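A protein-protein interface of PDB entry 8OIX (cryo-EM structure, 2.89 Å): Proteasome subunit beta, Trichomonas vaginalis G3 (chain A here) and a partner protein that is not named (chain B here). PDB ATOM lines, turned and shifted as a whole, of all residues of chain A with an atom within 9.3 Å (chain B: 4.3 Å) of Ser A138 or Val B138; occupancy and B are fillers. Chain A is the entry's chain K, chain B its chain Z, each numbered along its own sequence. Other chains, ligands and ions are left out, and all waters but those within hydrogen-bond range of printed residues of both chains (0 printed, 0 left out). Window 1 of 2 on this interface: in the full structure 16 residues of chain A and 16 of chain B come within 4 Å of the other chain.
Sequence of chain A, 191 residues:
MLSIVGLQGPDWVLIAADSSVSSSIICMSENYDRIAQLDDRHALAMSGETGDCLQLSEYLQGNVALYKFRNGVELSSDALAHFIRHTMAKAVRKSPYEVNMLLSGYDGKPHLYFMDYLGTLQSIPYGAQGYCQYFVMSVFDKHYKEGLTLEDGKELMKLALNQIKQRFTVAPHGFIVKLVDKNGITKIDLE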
ATOM      1  N   VAL A   5     -40.001 -12.778  23.353  1.00  0.00           N
ATOM      2  CA  VAL A   5     -38.715 -13.082  22.736  1.00  0.00           C
ATOM      3  C   VAL A   5     -38.946 -13.932  21.495  1.00  0.00           C
ATOM      4  O   VAL A   5     -39.584 -14.983  21.570  1.00  0.00           O
ATOM      5  CB  VAL A   5     -37.774 -13.814  23.712  1.00  0.00           C
ATOM      6  CG1 VAL A   5     -36.379 -13.878  23.144  1.00  0.00           C
ATOM      7  CG2 VAL A   5     -37.761 -13.125  25.058  1.00  0.00           C
ATOM      8  N   TYR A 126     -33.337 -12.717  15.558  1.00  0.00           N
ATOM      9  CA  TYR A 126     -33.804 -12.877  16.923  1.00  0.00           C
ATOM     10  C   TYR A 126     -34.017 -11.489  17.503  1.00  0.00           C
ATOM     11  O   TYR A 126     -33.448 -10.504  17.027  1.00  0.00           O
ATOM     12  CB  TYR A 126     -32.821 -13.689  17.768  1.00  0.00           C
ATOM     13  CG  TYR A 126     -31.373 -13.330  17.535  1.00  0.00           C
ATOM     14  CD1 TYR A 126     -30.840 -12.152  18.034  1.00  0.00           C
ATOM     15  CD2 TYR A 126     -30.537 -14.175  16.824  1.00  0.00           C
ATOM     16  CE1 TYR A 126     -29.521 -11.824  17.825  1.00  0.00           C
ATOM     17  CE2 TYR A 126     -29.215 -13.856  16.610  1.00  0.00           C
ATOM     18  CZ  TYR A 126     -28.712 -12.680  17.114  1.00  0.00           C
ATOM     19  OH  TYR A 126     -27.394 -12.355  16.904  1.00  0.00           O
ATOM     20  N   GLY A 127     -34.845 -11.424  18.533  1.00  0.00           N
ATOM     21  CA  GLY A 127     -35.174 -10.138  19.114  1.00  0.00           C
ATOM     22  C   GLY A 127     -36.087 -10.318  20.301  1.00  0.00           C
ATOM     23  O   GLY A 127     -36.459 -11.434  20.664  1.00  0.00           O
ATOM     24  N   ALA A 128     -36.435  -9.193  20.913  1.00  0.00           N
ATOM     25  CA  ALA A 128     -37.326  -9.230  22.059  1.00  0.00           C
ATOM     26  C   ALA A 128     -37.929  -7.853  22.278  1.00  0.00           C
ATOM     27  O   ALA A 128     -37.321  -6.833  21.952  1.00  0.00           O
ATOM     28  CB  ALA A 128     -36.594  -9.701  23.317  1.00  0.00           C
ATOM     29  N   CYS A 132     -36.726  -7.648  28.406  1.00  0.00           N
ATOM     30  CA  CYS A 132     -36.045  -8.924  28.230  1.00  0.00           C
ATOM     31  C   CYS A 132     -34.997  -8.866  27.135  1.00  0.00           C
ATOM     32  O   CYS A 132     -34.036  -9.641  27.167  1.00  0.00           O
ATOM     33  CB  CYS A 132     -37.052 -10.017  27.903  1.00  0.00           C
ATOM     34  SG  CYS A 132     -38.071  -9.644  26.475  1.00  0.00           S
ATOM     35  N   GLN A 133     -35.173  -7.985  26.148  1.00  0.00           N
ATOM     36  CA  GLN A 133     -34.158  -7.856  25.111  1.00  0.00           C
ATOM     37  C   GLN A 133     -32.812  -7.508  25.722  1.00  0.00           C
ATOM     38  O   GLN A 133     -31.793  -8.126  25.383  1.00  0.00           O
ATOM     39  CB  GLN A 133     -34.578  -6.804  24.086  1.00  0.00           C
ATOM     40  CG  GLN A 133     -35.543  -5.786  24.642  1.00  0.00           C
ATOM     41  CD  GLN A 133     -35.920  -4.702  23.653  1.00  0.00           C
ATOM     42  OE1 GLN A 133     -35.655  -4.814  22.456  1.00  0.00           O
ATOM     43  NE2 GLN A 133     -36.543  -3.641  24.150  1.00  0.00           N
ATOM     44  N   TYR A 134     -32.810  -6.626  26.729  1.00  0.00           N
ATOM     45  CA  TYR A 134     -31.556  -6.251  27.368  1.00  0.00           C
ATOM     46  C   TYR A 134     -30.844  -7.461  27.943  1.00  0.00           C
ATOM     47  O   TYR A 134     -29.621  -7.435  28.109  1.00  0.00           O
ATOM     48  CB  TYR A 134     -31.809  -5.215  28.463  1.00  0.00           C
ATOM     49  CG  TYR A 134     -32.312  -3.891  27.938  1.00  0.00           C
ATOM     50  CD1 TYR A 134     -31.436  -2.963  27.395  1.00  0.00           C
ATOM     51  CD2 TYR A 134     -33.661  -3.572  27.981  1.00  0.00           C
ATOM     52  CE1 TYR A 134     -31.887  -1.754  26.912  1.00  0.00           C
ATOM     53  CE2 TYR A 134     -34.121  -2.365  27.499  1.00  0.00           C
ATOM     54  CZ  TYR A 134     -33.230  -1.460  26.966  1.00  0.00           C
ATOM     55  OH  TYR A 134     -33.681  -0.253  26.483  1.00  0.00           O
ATOM     56  N   PHE A 135     -31.579  -8.537  28.196  1.00  0.00           N
ATOM     57  CA  PHE A 135     -31.035  -9.750  28.774  1.00  0.00           C
ATOM     58  C   PHE A 135     -30.846 -10.865  27.763  1.00  0.00           C
ATOM     59  O   PHE A 135     -30.019 -11.747  27.998  1.00  0.00           O
ATOM     60  CB  PHE A 135     -31.946 -10.256  29.899  1.00  0.00           C
ATOM     61  CG  PHE A 135     -32.142  -9.269  31.008  1.00  0.00           C
ATOM     62  CD1 PHE A 135     -31.256  -9.217  32.069  1.00  0.00           C
ATOM     63  CD2 PHE A 135     -33.213  -8.394  30.993  1.00  0.00           C
ATOM     64  CE1 PHE A 135     -31.436  -8.311  33.092  1.00  0.00           C
ATOM     65  CE2 PHE A 135     -33.396  -7.486  32.012  1.00  0.00           C
ATOM     66  CZ  PHE A 135     -32.507  -7.446  33.064  1.00  0.00           C
ATOM     67  N   VAL A 136     -31.583 -10.862  26.651  1.00  0.00           N
ATOM     68  CA  VAL A 136     -31.567 -12.039  25.786  1.00  0.00           C
ATOM     69  C   VAL A 136     -30.770 -11.808  24.512  1.00  0.00           C
ATOM     70  O   VAL A 136     -30.163 -12.744  23.979  1.00  0.00           O
ATOM     71  CB  VAL A 136     -32.994 -12.504  25.437  1.00  0.00           C
ATOM     72  CG1 VAL A 136     -33.771 -12.792  26.691  1.00  0.00           C
ATOM     73  CG2 VAL A 136     -33.710 -11.475  24.582  1.00  0.00           C
ATOM     74  N   MET A 137     -30.716 -10.559  24.045  1.00  0.00           N
ATOM     75  CA  MET A 137     -30.033 -10.288  22.786  1.00  0.00           C
ATOM     76  C   MET A 137     -28.595 -10.775  22.836  1.00  0.00           C
ATOM     77  O   MET A 137     -28.158 -11.540  21.964  1.00  0.00           O
ATOM     78  CB  MET A 137     -30.079  -8.792  22.480  1.00  0.00           C
ATOM     79  CG  MET A 137     -31.479  -8.237  22.289  1.00  0.00           C
ATOM     80  SD  MET A 137     -32.496  -9.194  21.157  1.00  0.00           S
ATOM     81  CE  MET A 137     -31.488  -9.161  19.679  1.00  0.00           C
ATOM     82  N   SER A 138     -27.889 -10.452  23.921  1.00  0.00           N
ATOM     83  CA  SER A 138     -26.509 -10.889  24.056  1.00  0.00           C
ATOM     84  C   SER A 138     -26.411 -12.403  24.009  1.00  0.00           C
ATOM     85  O   SER A 138     -25.567 -12.949  23.286  1.00  0.00           O
ATOM     86  CB  SER A 138     -25.912 -10.361  25.356  1.00  0.00           C
ATOM     87  OG  SER A 138     -26.607 -10.876  26.478  1.00  0.00           O
ATOM     88  N   VAL A 139     -27.306 -13.103  24.714  1.00  0.00           N
ATOM     89  CA  VAL A 139     -27.209 -14.558  24.715  1.00  0.00           C
ATOM     90  C   VAL A 139     -27.403 -15.074  23.299  1.00  0.00           C
ATOM     91  O   VAL A 139     -26.639 -15.927  22.827  1.00  0.00           O
ATOM     92  CB  VAL A 139     -28.191 -15.189  25.728  1.00  0.00           C
ATOM     93  CG1 VAL A 139     -28.334 -14.309  26.959  1.00  0.00           C
ATOM     94  CG2 VAL A 139     -29.549 -15.520  25.121  1.00  0.00           C
ATOM     95  N   PHE A 140     -28.355 -14.492  22.562  1.00  0.00           N
ATOM     96  CA  PHE A 140     -28.509 -14.869  21.165  1.00  0.00           C
ATOM     97  C   PHE A 140     -27.220 -14.594  20.414  1.00  0.00           C
ATOM     98  O   PHE A 140     -26.649 -15.493  19.783  1.00  0.00           O
ATOM     99  CB  PHE A 140     -29.676 -14.112  20.540  1.00  0.00           C
ATOM    100  CG  PHE A 140     -31.019 -14.562  21.022  1.00  0.00           C
ATOM    101  CD1 PHE A 140     -31.271 -15.901  21.255  1.00  0.00           C
ATOM    102  CD2 PHE A 140     -32.033 -13.648  21.237  1.00  0.00           C
ATOM    103  CE1 PHE A 140     -32.506 -16.320  21.696  1.00  0.00           C
ATOM    104  CE2 PHE A 140     -33.269 -14.061  21.676  1.00  0.00           C
ATOM    105  CZ  PHE A 140     -33.505 -15.400  21.907  1.00  0.00           C
ATOM    106  N   ASP A 141     -26.693 -13.377  20.565  1.00  0.00           N
ATOM    107  CA  ASP A 141     -25.442 -13.028  19.909  1.00  0.00           C
ATOM    108  C   ASP A 141     -24.348 -14.003  20.306  1.00  0.00           C
ATOM    109  O   ASP A 141     -23.495 -14.363  19.487  1.00  0.00           O
ATOM    110  CB  ASP A 141     -25.042 -11.597  20.266  1.00  0.00           C
ATOM    111  CG  ASP A 141     -26.061 -10.576  19.810  1.00  0.00           C
ATOM    112  OD1 ASP A 141     -26.852 -10.892  18.902  1.00  0.00           O
ATOM    113  OD2 ASP A 141     -26.068  -9.457  20.360  1.00  0.00           O
ATOM    114  N   LYS A 142     -24.360 -14.444  21.563  1.00  0.00           N
ATOM    115  CA  LYS A 142     -23.297 -15.319  22.022  1.00  0.00           C
ATOM    116  C   LYS A 142     -23.481 -16.741  21.511  1.00  0.00           C
ATOM    117  O   LYS A 142     -22.490 -17.442  21.278  1.00  0.00           O
ATOM    118  CB  LYS A 142     -23.225 -15.295  23.550  1.00  0.00           C
ATOM    119  CG  LYS A 142     -22.115 -16.143  24.135  1.00  0.00           C
ATOM    120  CD  LYS A 142     -20.761 -15.696  23.618  1.00  0.00           C
ATOM    121  CE  LYS A 142     -19.629 -16.407  24.335  1.00  0.00           C
ATOM    122  NZ  LYS A 142     -19.774 -17.888  24.264  1.00  0.00           N
ATOM    123  N   HIS A 143     -24.726 -17.181  21.310  1.00  0.00           N
ATOM    124  CA  HIS A 143     -24.983 -18.594  21.070  1.00  0.00           C
ATOM    125  C   HIS A 143     -25.735 -18.910  19.786  1.00  0.00           C
ATOM    126  O   HIS A 143     -25.950 -20.093  19.499  1.00  0.00           O
ATOM    127  CB  HIS A 143     -25.740 -19.195  22.259  1.00  0.00           C
ATOM    128  CG  HIS A 143     -24.958 -19.181  23.533  1.00  0.00           C
ATOM    129  ND1 HIS A 143     -24.176 -20.241  23.937  1.00  0.00           N
ATOM    130  CD2 HIS A 143     -24.829 -18.233  24.491  1.00  0.00           C
ATOM    131  CE1 HIS A 143     -23.601 -19.949  25.089  1.00  0.00           C
ATOM    132  NE2 HIS A 143     -23.977 -18.734  25.445  1.00  0.00           N
ATOM    133  N   TYR A 144     -26.142 -17.917  19.004  1.00  0.00           N
ATOM    134  CA  TYR A 144     -26.864 -18.210  17.775  1.00  0.00           C
ATOM    135  C   TYR A 144     -25.885 -18.536  16.657  1.00  0.00           C
ATOM    136  O   TYR A 144     -24.932 -17.791  16.414  1.00  0.00           O
ATOM    137  CB  TYR A 144     -27.758 -17.042  17.368  1.00  0.00           C
ATOM    138  CG  TYR A 144     -28.670 -17.363  16.207  1.00  0.00           C
ATOM    139  CD1 TYR A 144     -28.274 -17.132  14.898  1.00  0.00           C
ATOM    140  CD2 TYR A 144     -29.920 -17.919  16.421  1.00  0.00           C
ATOM    141  CE1 TYR A 144     -29.105 -17.435  13.838  1.00  0.00           C
ATOM    142  CE2 TYR A 144     -30.758 -18.222  15.366  1.00  0.00           C
ATOM    143  CZ  TYR A 144     -30.347 -17.976  14.077  1.00  0.00           C
ATOM    144  OH  TYR A 144     -31.178 -18.279  13.026  1.00  0.00           O
ATOM    145  N   LEU A 156     -31.541 -22.621  22.829  1.00  0.00           N
ATOM    146  CA  LEU A 156     -31.172 -21.209  22.885  1.00  0.00           C
ATOM    147  C   LEU A 156     -32.312 -20.350  23.419  1.00  0.00           C
ATOM    148  O   LEU A 156     -32.085 -19.432  24.217  1.00  0.00           O
ATOM    149  CB  LEU A 156     -30.740 -20.735  21.498  1.00  0.00           C
ATOM    150  CG  LEU A 156     -30.335 -19.268  21.366  1.00  0.00           C
ATOM    151  CD1 LEU A 156     -29.291 -18.903  22.402  1.00  0.00           C
ATOM    152  CD2 LEU A 156     -29.820 -18.987  19.965  1.00  0.00           C
ATOM    153  N   LEU A 159     -32.408 -20.871  27.051  1.00  0.00           N
ATOM    154  CA  LEU A 159     -31.345 -20.093  27.678  1.00  0.00           C
ATOM    155  C   LEU A 159     -31.750 -18.633  27.829  1.00  0.00           C
ATOM    156  O   LEU A 159     -31.521 -18.020  28.878  1.00  0.00           O
ATOM    157  CB  LEU A 159     -30.067 -20.215  26.850  1.00  0.00           C
ATOM    158  CG  LEU A 159     -28.994 -21.180  27.346  1.00  0.00           C
ATOM    159  CD1 LEU A 159     -29.598 -22.539  27.645  1.00  0.00           C
ATOM    160  CD2 LEU A 159     -27.922 -21.316  26.285  1.00  0.00           C
ATOM    161  N   ALA A 160     -32.359 -18.061  26.789  1.00  0.00           N
ATOM    162  CA  ALA A 160     -32.787 -16.666  26.850  1.00  0.00           C
ATOM    163  C   ALA A 160     -33.864 -16.468  27.912  1.00  0.00           C
ATOM    164  O   ALA A 160     -33.822 -15.505  28.690  1.00  0.00           O
ATOM    165  CB  ALA A 160     -33.287 -16.214  25.479  1.00  0.00           C
ATOM    166  N   GLN A 163     -32.393 -16.610  31.263  1.00  0.00           N
ATOM    167  CA  GLN A 163     -31.746 -15.341  31.579  1.00  0.00           C
ATOM    168  C   GLN A 163     -32.764 -14.296  32.012  1.00  0.00           C
ATOM    169  O   GLN A 163     -32.505 -13.514  32.934  1.00  0.00           O
ATOM    170  CB  GLN A 163     -30.942 -14.839  30.383  1.00  0.00           C
ATOM    171  CG  GLN A 163     -29.490 -15.225  30.461  1.00  0.00           C
ATOM    172  CD  GLN A 163     -28.885 -14.833  31.788  1.00  0.00           C
ATOM    173  OE1 GLN A 163     -28.608 -15.687  32.626  1.00  0.00           O
ATOM    174  NE2 GLN A 163     -28.702 -13.537  32.000  1.00  0.00           N
ATOM    175  N   GLN A 166     -33.687 -15.213  35.580  1.00  0.00           N
ATOM    176  CA  GLN A 166     -32.647 -15.077  36.592  1.00  0.00           C
ATOM    177  C   GLN A 166     -32.230 -13.626  36.809  1.00  0.00           C
ATOM    178  O   GLN A 166     -32.052 -13.200  37.955  1.00  0.00           O
ATOM    179  CB  GLN A 166     -31.433 -15.924  36.207  1.00  0.00           C
ATOM    180  CG  GLN A 166     -30.309 -15.895  37.229  1.00  0.00           C
ATOM    181  CD  GLN A 166     -29.065 -16.616  36.749  1.00  0.00           C
ATOM    182  OE1 GLN A 166     -28.344 -16.125  35.882  1.00  0.00           O
ATOM    183  NE2 GLN A 166     -28.806 -17.789  37.316  1.00  0.00           N
ATOM    184  N   ARG A 167     -32.064 -12.850  35.736  1.00  0.00           N
ATOM    185  CA  ARG A 167     -31.495 -11.516  35.868  1.00  0.00           C
ATOM    186  C   ARG A 167     -32.518 -10.389  35.828  1.00  0.00           C
ATOM    187  O   ARG A 167     -32.246  -9.318  36.380  1.00  0.00           O
ATOM    188  CB  ARG A 167     -30.455 -11.275  34.771  1.00  0.00           C
ATOM    189  CG  ARG A 167     -29.186 -12.073  34.956  1.00  0.00           C
ATOM    190  CD  ARG A 167     -28.509 -11.729  36.269  1.00  0.00           C
ATOM    191  NE  ARG A 167     -27.353 -12.581  36.517  1.00  0.00           N
ATOM    192  CZ  ARG A 167     -26.704 -12.644  37.670  1.00  0.00           C
ATOM    193  NH1 ARG A 167     -27.080 -11.927  38.714  1.00  0.00           N
ATOM    194  NH2 ARG A 167     -25.651 -13.451  37.779  1.00  0.00           N
ATOM    195  N   HIS B 134     -26.503  -7.220  29.139  1.00  0.00           N
ATOM    196  CA  HIS B 134     -25.952  -8.079  28.096  1.00  0.00           C
ATOM    197  C   HIS B 134     -24.723  -8.833  28.589  1.00  0.00           C
ATOM    198  O   HIS B 134     -24.561 -10.032  28.311  1.00  0.00           O
ATOM    199  CB  HIS B 134     -25.611  -7.235  26.872  1.00  0.00           C
ATOM    200  CG  HIS B 134     -26.733  -6.355  26.426  1.00  0.00           C
ATOM    201  ND1 HIS B 134     -26.779  -5.008  26.711  1.00  0.00           N
ATOM    202  CD2 HIS B 134     -27.864  -6.634  25.740  1.00  0.00           C
ATOM    203  CE1 HIS B 134     -27.885  -4.492  26.205  1.00  0.00           C
ATOM    204  NE2 HIS B 134     -28.560  -5.458  25.611  1.00  0.00           N
ATOM    205  N   ALA B 135     -23.841  -8.142  29.313  1.00  0.00           N
ATOM    206  CA  ALA B 135     -22.694  -8.809  29.913  1.00  0.00           C
ATOM    207  C   ALA B 135     -23.147  -9.887  30.883  1.00  0.00           C
ATOM    208  O   ALA B 135     -22.559 -10.969  30.937  1.00  0.00           O
ATOM    209  CB  ALA B 135     -21.800  -7.790  30.616  1.00  0.00           C
ATOM    210  N   TYR B 136     -24.204  -9.610  31.649  1.00  0.00           N
ATOM    211  CA  TYR B 136     -24.764 -10.611  32.549  1.00  0.00           C
ATOM    212  C   TYR B 136     -25.298 -11.811  31.785  1.00  0.00           C
ATOM    213  O   TYR B 136     -25.107 -12.954  32.206  1.00  0.00           O
ATOM    214  CB  TYR B 136     -25.882  -9.993  33.384  1.00  0.00           C
ATOM    215  CG  TYR B 136     -25.519  -9.682  34.813  1.00  0.00           C
ATOM    216  CD1 TYR B 136     -24.717 -10.537  35.551  1.00  0.00           C
ATOM    217  CD2 TYR B 136     -26.000  -8.541  35.431  1.00  0.00           C
ATOM    218  CE1 TYR B 136     -24.400 -10.258  36.865  1.00  0.00           C
ATOM    219  CE2 TYR B 136     -25.690  -8.254  36.739  1.00  0.00           C
ATOM    220  CZ  TYR B 136     -24.891  -9.114  37.451  1.00  0.00           C
ATOM    221  OH  TYR B 136     -24.589  -8.819  38.758  1.00  0.00           O
ATOM    222  N   GLY B 137     -25.993 -11.575  30.674  1.00  0.00           N
ATOM    223  CA  GLY B 137     -26.475 -12.690  29.880  1.00  0.00           C
ATOM    224  C   GLY B 137     -25.352 -13.572  29.375  1.00  0.00           C
ATOM    225  O   GLY B 137     -25.381 -14.795  29.555  1.00  0.00           O
ATOM    226  N   VAL B 138     -24.297 -12.954  28.838  1.00  0.00           N
ATOM    227  CA  VAL B 138     -23.172 -13.737  28.335  1.00  0.00           C
ATOM    228  C   VAL B 138     -22.474 -14.471  29.473  1.00  0.00           C
ATOM    229  O   VAL B 138     -22.125 -15.650  29.342  1.00  0.00           O
ATOM    230  CB  VAL B 138     -22.193 -12.847  27.551  1.00  0.00           C
ATOM    231  CG1 VAL B 138     -20.976 -13.656  27.132  1.00  0.00           C
ATOM    232  CG2 VAL B 138     -22.876 -12.249  26.337  1.00  0.00           C
ATOM    233  N   LEU B 139     -22.259 -13.796  30.603  1.00  0.00           N
ATOM    234  CA  LEU B 139     -21.597 -14.436  31.733  1.00  0.00           C
ATOM    235  C   LEU B 139     -22.413 -15.622  32.224  1.00  0.00           C
ATOM    236  O   LEU B 139     -21.977 -16.774  32.133  1.00  0.00           O
ATOM    237  CB  LEU B 139     -21.385 -13.429  32.866  1.00  0.00           C
ATOM    238  CG  LEU B 139     -20.358 -12.312  32.680  1.00  0.00           C
ATOM    239  CD1 LEU B 139     -20.315 -11.423  33.913  1.00  0.00           C
ATOM    240  CD2 LEU B 139     -18.987 -12.879  32.373  1.00  0.00           C
ATOM    241  N   ASP B 140     -23.631 -15.357  32.704  1.00  0.00           N
ATOM    242  CA  ASP B 140     -24.457 -16.405  33.290  1.00  0.00           C
ATOM    243  C   ASP B 140     -24.698 -17.547  32.317  1.00  0.00           C
ATOM    244  O   ASP B 140     -24.962 -18.676  32.746  1.00  0.00           O
ATOM    245  CB  ASP B 140     -25.788 -15.826  33.757  1.00  0.00           C
ATOM    246  CG  ASP B 140     -25.619 -14.591  34.608  1.00  0.00           C
ATOM    247  OD1 ASP B 140     -24.527 -14.402  35.176  1.00  0.00           O
ATOM    248  OD2 ASP B 140     -26.579 -13.805  34.705  1.00  0.00           O
ATOM    249  N   THR B 141     -24.617 -17.289  31.012  1.00  0.00           N
ATOM    250  CA  THR B 141     -24.810 -18.375  30.068  1.00  0.00           C
ATOM    251  C   THR B 141     -23.529 -19.160  29.809  1.00  0.00           C
ATOM    252  O   THR B 141     -23.591 -20.376  29.596  1.00  0.00           O
ATOM    253  CB  THR B 141     -25.361 -17.829  28.750  1.00  0.00           C
ATOM    254  OG1 THR B 141     -26.411 -16.893  29.026  1.00  0.00           O
ATOM    255  CG2 THR B 141     -25.934 -18.952  27.928  1.00  0.00           C
ATOM    256  N   CYS B 142     -22.370 -18.501  29.829  1.00  0.00           N
ATOM    257  CA  CYS B 142     -21.101 -19.149  29.523  1.00  0.00           C
ATOM    258  C   CYS B 142     -20.166 -19.297  30.718  1.00  0.00           C
ATOM    259  O   CYS B 142     -19.071 -19.844  30.556  1.00  0.00           O
ATOM    260  CB  CYS B 142     -20.381 -18.384  28.410  1.00  0.00           C
ATOM    261  SG  CYS B 142     -21.415 -18.055  26.975  1.00  0.00           S
ATOM    262  N   LEU B 155     -14.094 -14.986  28.405  1.00  0.00           N
ATOM    263  CA  LEU B 155     -15.505 -14.882  28.758  1.00  0.00           C
ATOM    264  C   LEU B 155     -15.869 -13.450  29.120  1.00  0.00           C
ATOM    265  O   LEU B 155     -16.864 -12.905  28.628  1.00  0.00           O
ATOM    266  CB  LEU B 155     -15.825 -15.817  29.922  1.00  0.00           C
ATOM    267  CG  LEU B 155     -17.130 -15.518  30.669  1.00  0.00           C
ATOM    268  CD1 LEU B 155     -18.344 -15.624  29.752  1.00  0.00           C
ATOM    269  CD2 LEU B 155     -17.283 -16.407  31.887  1.00  0.00           C
ATOM    270  N   ARG B 158     -15.711 -11.270  25.961  1.00  0.00           N
ATOM    271  CA  ARG B 158     -16.827 -11.462  25.045  1.00  0.00           C
ATOM    272  C   ARG B 158     -18.128 -10.935  25.627  1.00  0.00           C
ATOM    273  O   ARG B 158     -18.973 -10.430  24.884  1.00  0.00           O
ATOM    274  CB  ARG B 158     -16.967 -12.941  24.687  1.00  0.00           C
ATOM    275  CG  ARG B 158     -15.940 -13.429  23.687  1.00  0.00           C
ATOM    276  CD  ARG B 158     -16.223 -12.865  22.307  1.00  0.00           C
ATOM    277  NE  ARG B 158     -15.018 -12.778  21.493  1.00  0.00           N
ATOM    278  CZ  ARG B 158     -14.978 -12.269  20.269  1.00  0.00           C
ATOM    279  NH1 ARG B 158     -16.062 -11.788  19.685  1.00  0.00           N
ATOM    280  NH2 ARG B 158     -13.821 -12.246  19.614  1.00  0.00           N
ATOM    281  N   ALA B 159     -18.311 -11.038  26.944  1.00  0.00           N
ATOM    282  CA  ALA B 159     -19.487 -10.437  27.558  1.00  0.00           C
ATOM    283  C   ALA B 159     -19.474  -8.924  27.395  1.00  0.00           C
ATOM    284  O   ALA B 159     -20.497  -8.319  27.048  1.00  0.00           O
ATOM    285  CB  ALA B 159     -19.572 -10.833  29.029  1.00  0.00           C
ATOM    286  N   HIS B 162     -20.311  -8.171  23.711  1.00  0.00           N
ATOM    287  CA  HIS B 162     -21.728  -8.264  23.388  1.00  0.00           C
ATOM    288  C   HIS B 162     -22.510  -7.118  24.012  1.00  0.00           C
ATOM    289  O   HIS B 162     -23.473  -6.623  23.413  1.00  0.00           O
ATOM    290  CB  HIS B 162     -22.291  -9.610  23.840  1.00  0.00           C
ATOM    291  CG  HIS B 162     -21.824 -10.767  23.014  1.00  0.00           C
ATOM    292  ND1 HIS B 162     -22.232 -10.963  21.713  1.00  0.00           N
ATOM    293  CD2 HIS B 162     -20.996 -11.798  23.306  1.00  0.00           C
ATOM    294  CE1 HIS B 162     -21.666 -12.057  21.235  1.00  0.00           C
ATOM    295  NE2 HIS B 162     -20.911 -12.582  22.182  1.00  0.00           N
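Printed residues of chain B that touch a printed residue of chain A: His B134, Tyr B136, Gly B137, Val B138, Asp B140, Thr B141, Cys B142 and His B162.
Hydrophobic or aromatic side chains of chain B that line the printed part of chain A: His B134, Tyr B136, Val B138 and His B162.
Hydrophobic or aromatic side chains of chain A within 4 Å of the printed part of chain B: Val A139, His A143 and Leu A159.
Among the printed residues, 20 pairs touch across the chains.
Among the printed residues, Asp or Glu carboxylates within 4 Å of a Lys or Arg side-chain nitrogen of the other chain: Arg A167 with Asp B140.
The backbone NH (N) of His B134 lies close to the backbone carbonyl oxygen (O) of Tyr A134 (3.3 Å).
The backbone carbonyl oxygen (O) of His B134 lies within hydrogen-bond range of the side-chain hydroxyl (OG) of Ser A138 (2.9 Å).
The side-chain amino group of Lys A142 is in hydrogen-bond range of the side-chain sulfur of Cys B142, 3.2 Å away.
The side-chain sulfur (SG) of Cys B142 lies within hydrogen-bond range of a ring nitrogen (NE2) of His A143 (3.1 Å).
The side-chain amide nitrogen (NE2) of Gln A163 is in hydrogen-bond range of the side-chain carboxylate (OD2) of Asp B140.
OE1 of Gln A166 sits close to OD2 of Asp B140, at 3.1 Å.
The side-chain carboxylate of Asp B140 lies within salt-bridge range of the guanidinium group of Arg A167, 3.0 Å away.
Gly B137 touches Ser A138 (CA to OG, 3.9 Å).
Ser A138 touches Val B138.
His B162 touches Ser A138.
Gly B137 touches Val A139 (CA to CG1, 3.8 Å).
CD of Lys A142 touches NE2 of His B162, at 3.4 Å.
NE2 of His A143 touches CG2 of Thr B141, 3.2 Å away.
Leu A159 touches Thr B141.
NE2 of Gln A163 touches CA of Gly B137, 3.2 Å away.
OG1 of Thr B141 touches CG of Gln A163, 3.8 Å away.
Arg A167 touches Tyr B136 (CZ to CE1, 3.4 Å).
The side-chain hydroxyl (OH) of Tyr A126 is in hydrogen-bond range of the side-chain carboxylate (OD1) of Asp A141 (2.5 Å).
The side-chain amide oxygen (OE1) of Gln A163 lies close to the side-chain amide oxygen (OE1) of Gln A166 (3.3 Å).
O of Val B138 sits close to SG of Cys B142, 3.4 Å away.
Cys A132 touches none of the printed residues of chain B.
Gln A133 touches none of the printed residues of chain B.
Printed residues of chain B within 4 Å of Ser A138: His B134 (2.9 Å), Gly B137 (3.9 Å), Val B138 (3.7 Å) and His B162 (3.997 Å).
Printed residues of chain B within 4 Å of Gln A163: Tyr B136, Gly B137, Asp B140 and Thr B141.
Printed residues of chain A within 4 Å of Tyr B136: Gln A163 (3.6 Å) and Arg A167 (3.4 Å).
Of chain A, only Ser A138 comes within 4 Å of Val B138.
Of chain A, only Val A139, His A143, Leu A159 and Gln A163 come within 4 Å of Thr B141.
No residue of chain A comes within 4 Å of Ala B159.
The nearest printed residue of chain B that does not touch Ser A138 is Ala B135 (4.8 Å).
The nearest residue of chain A that does not touch Val B138 is Lys A142 (4.1 Å).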
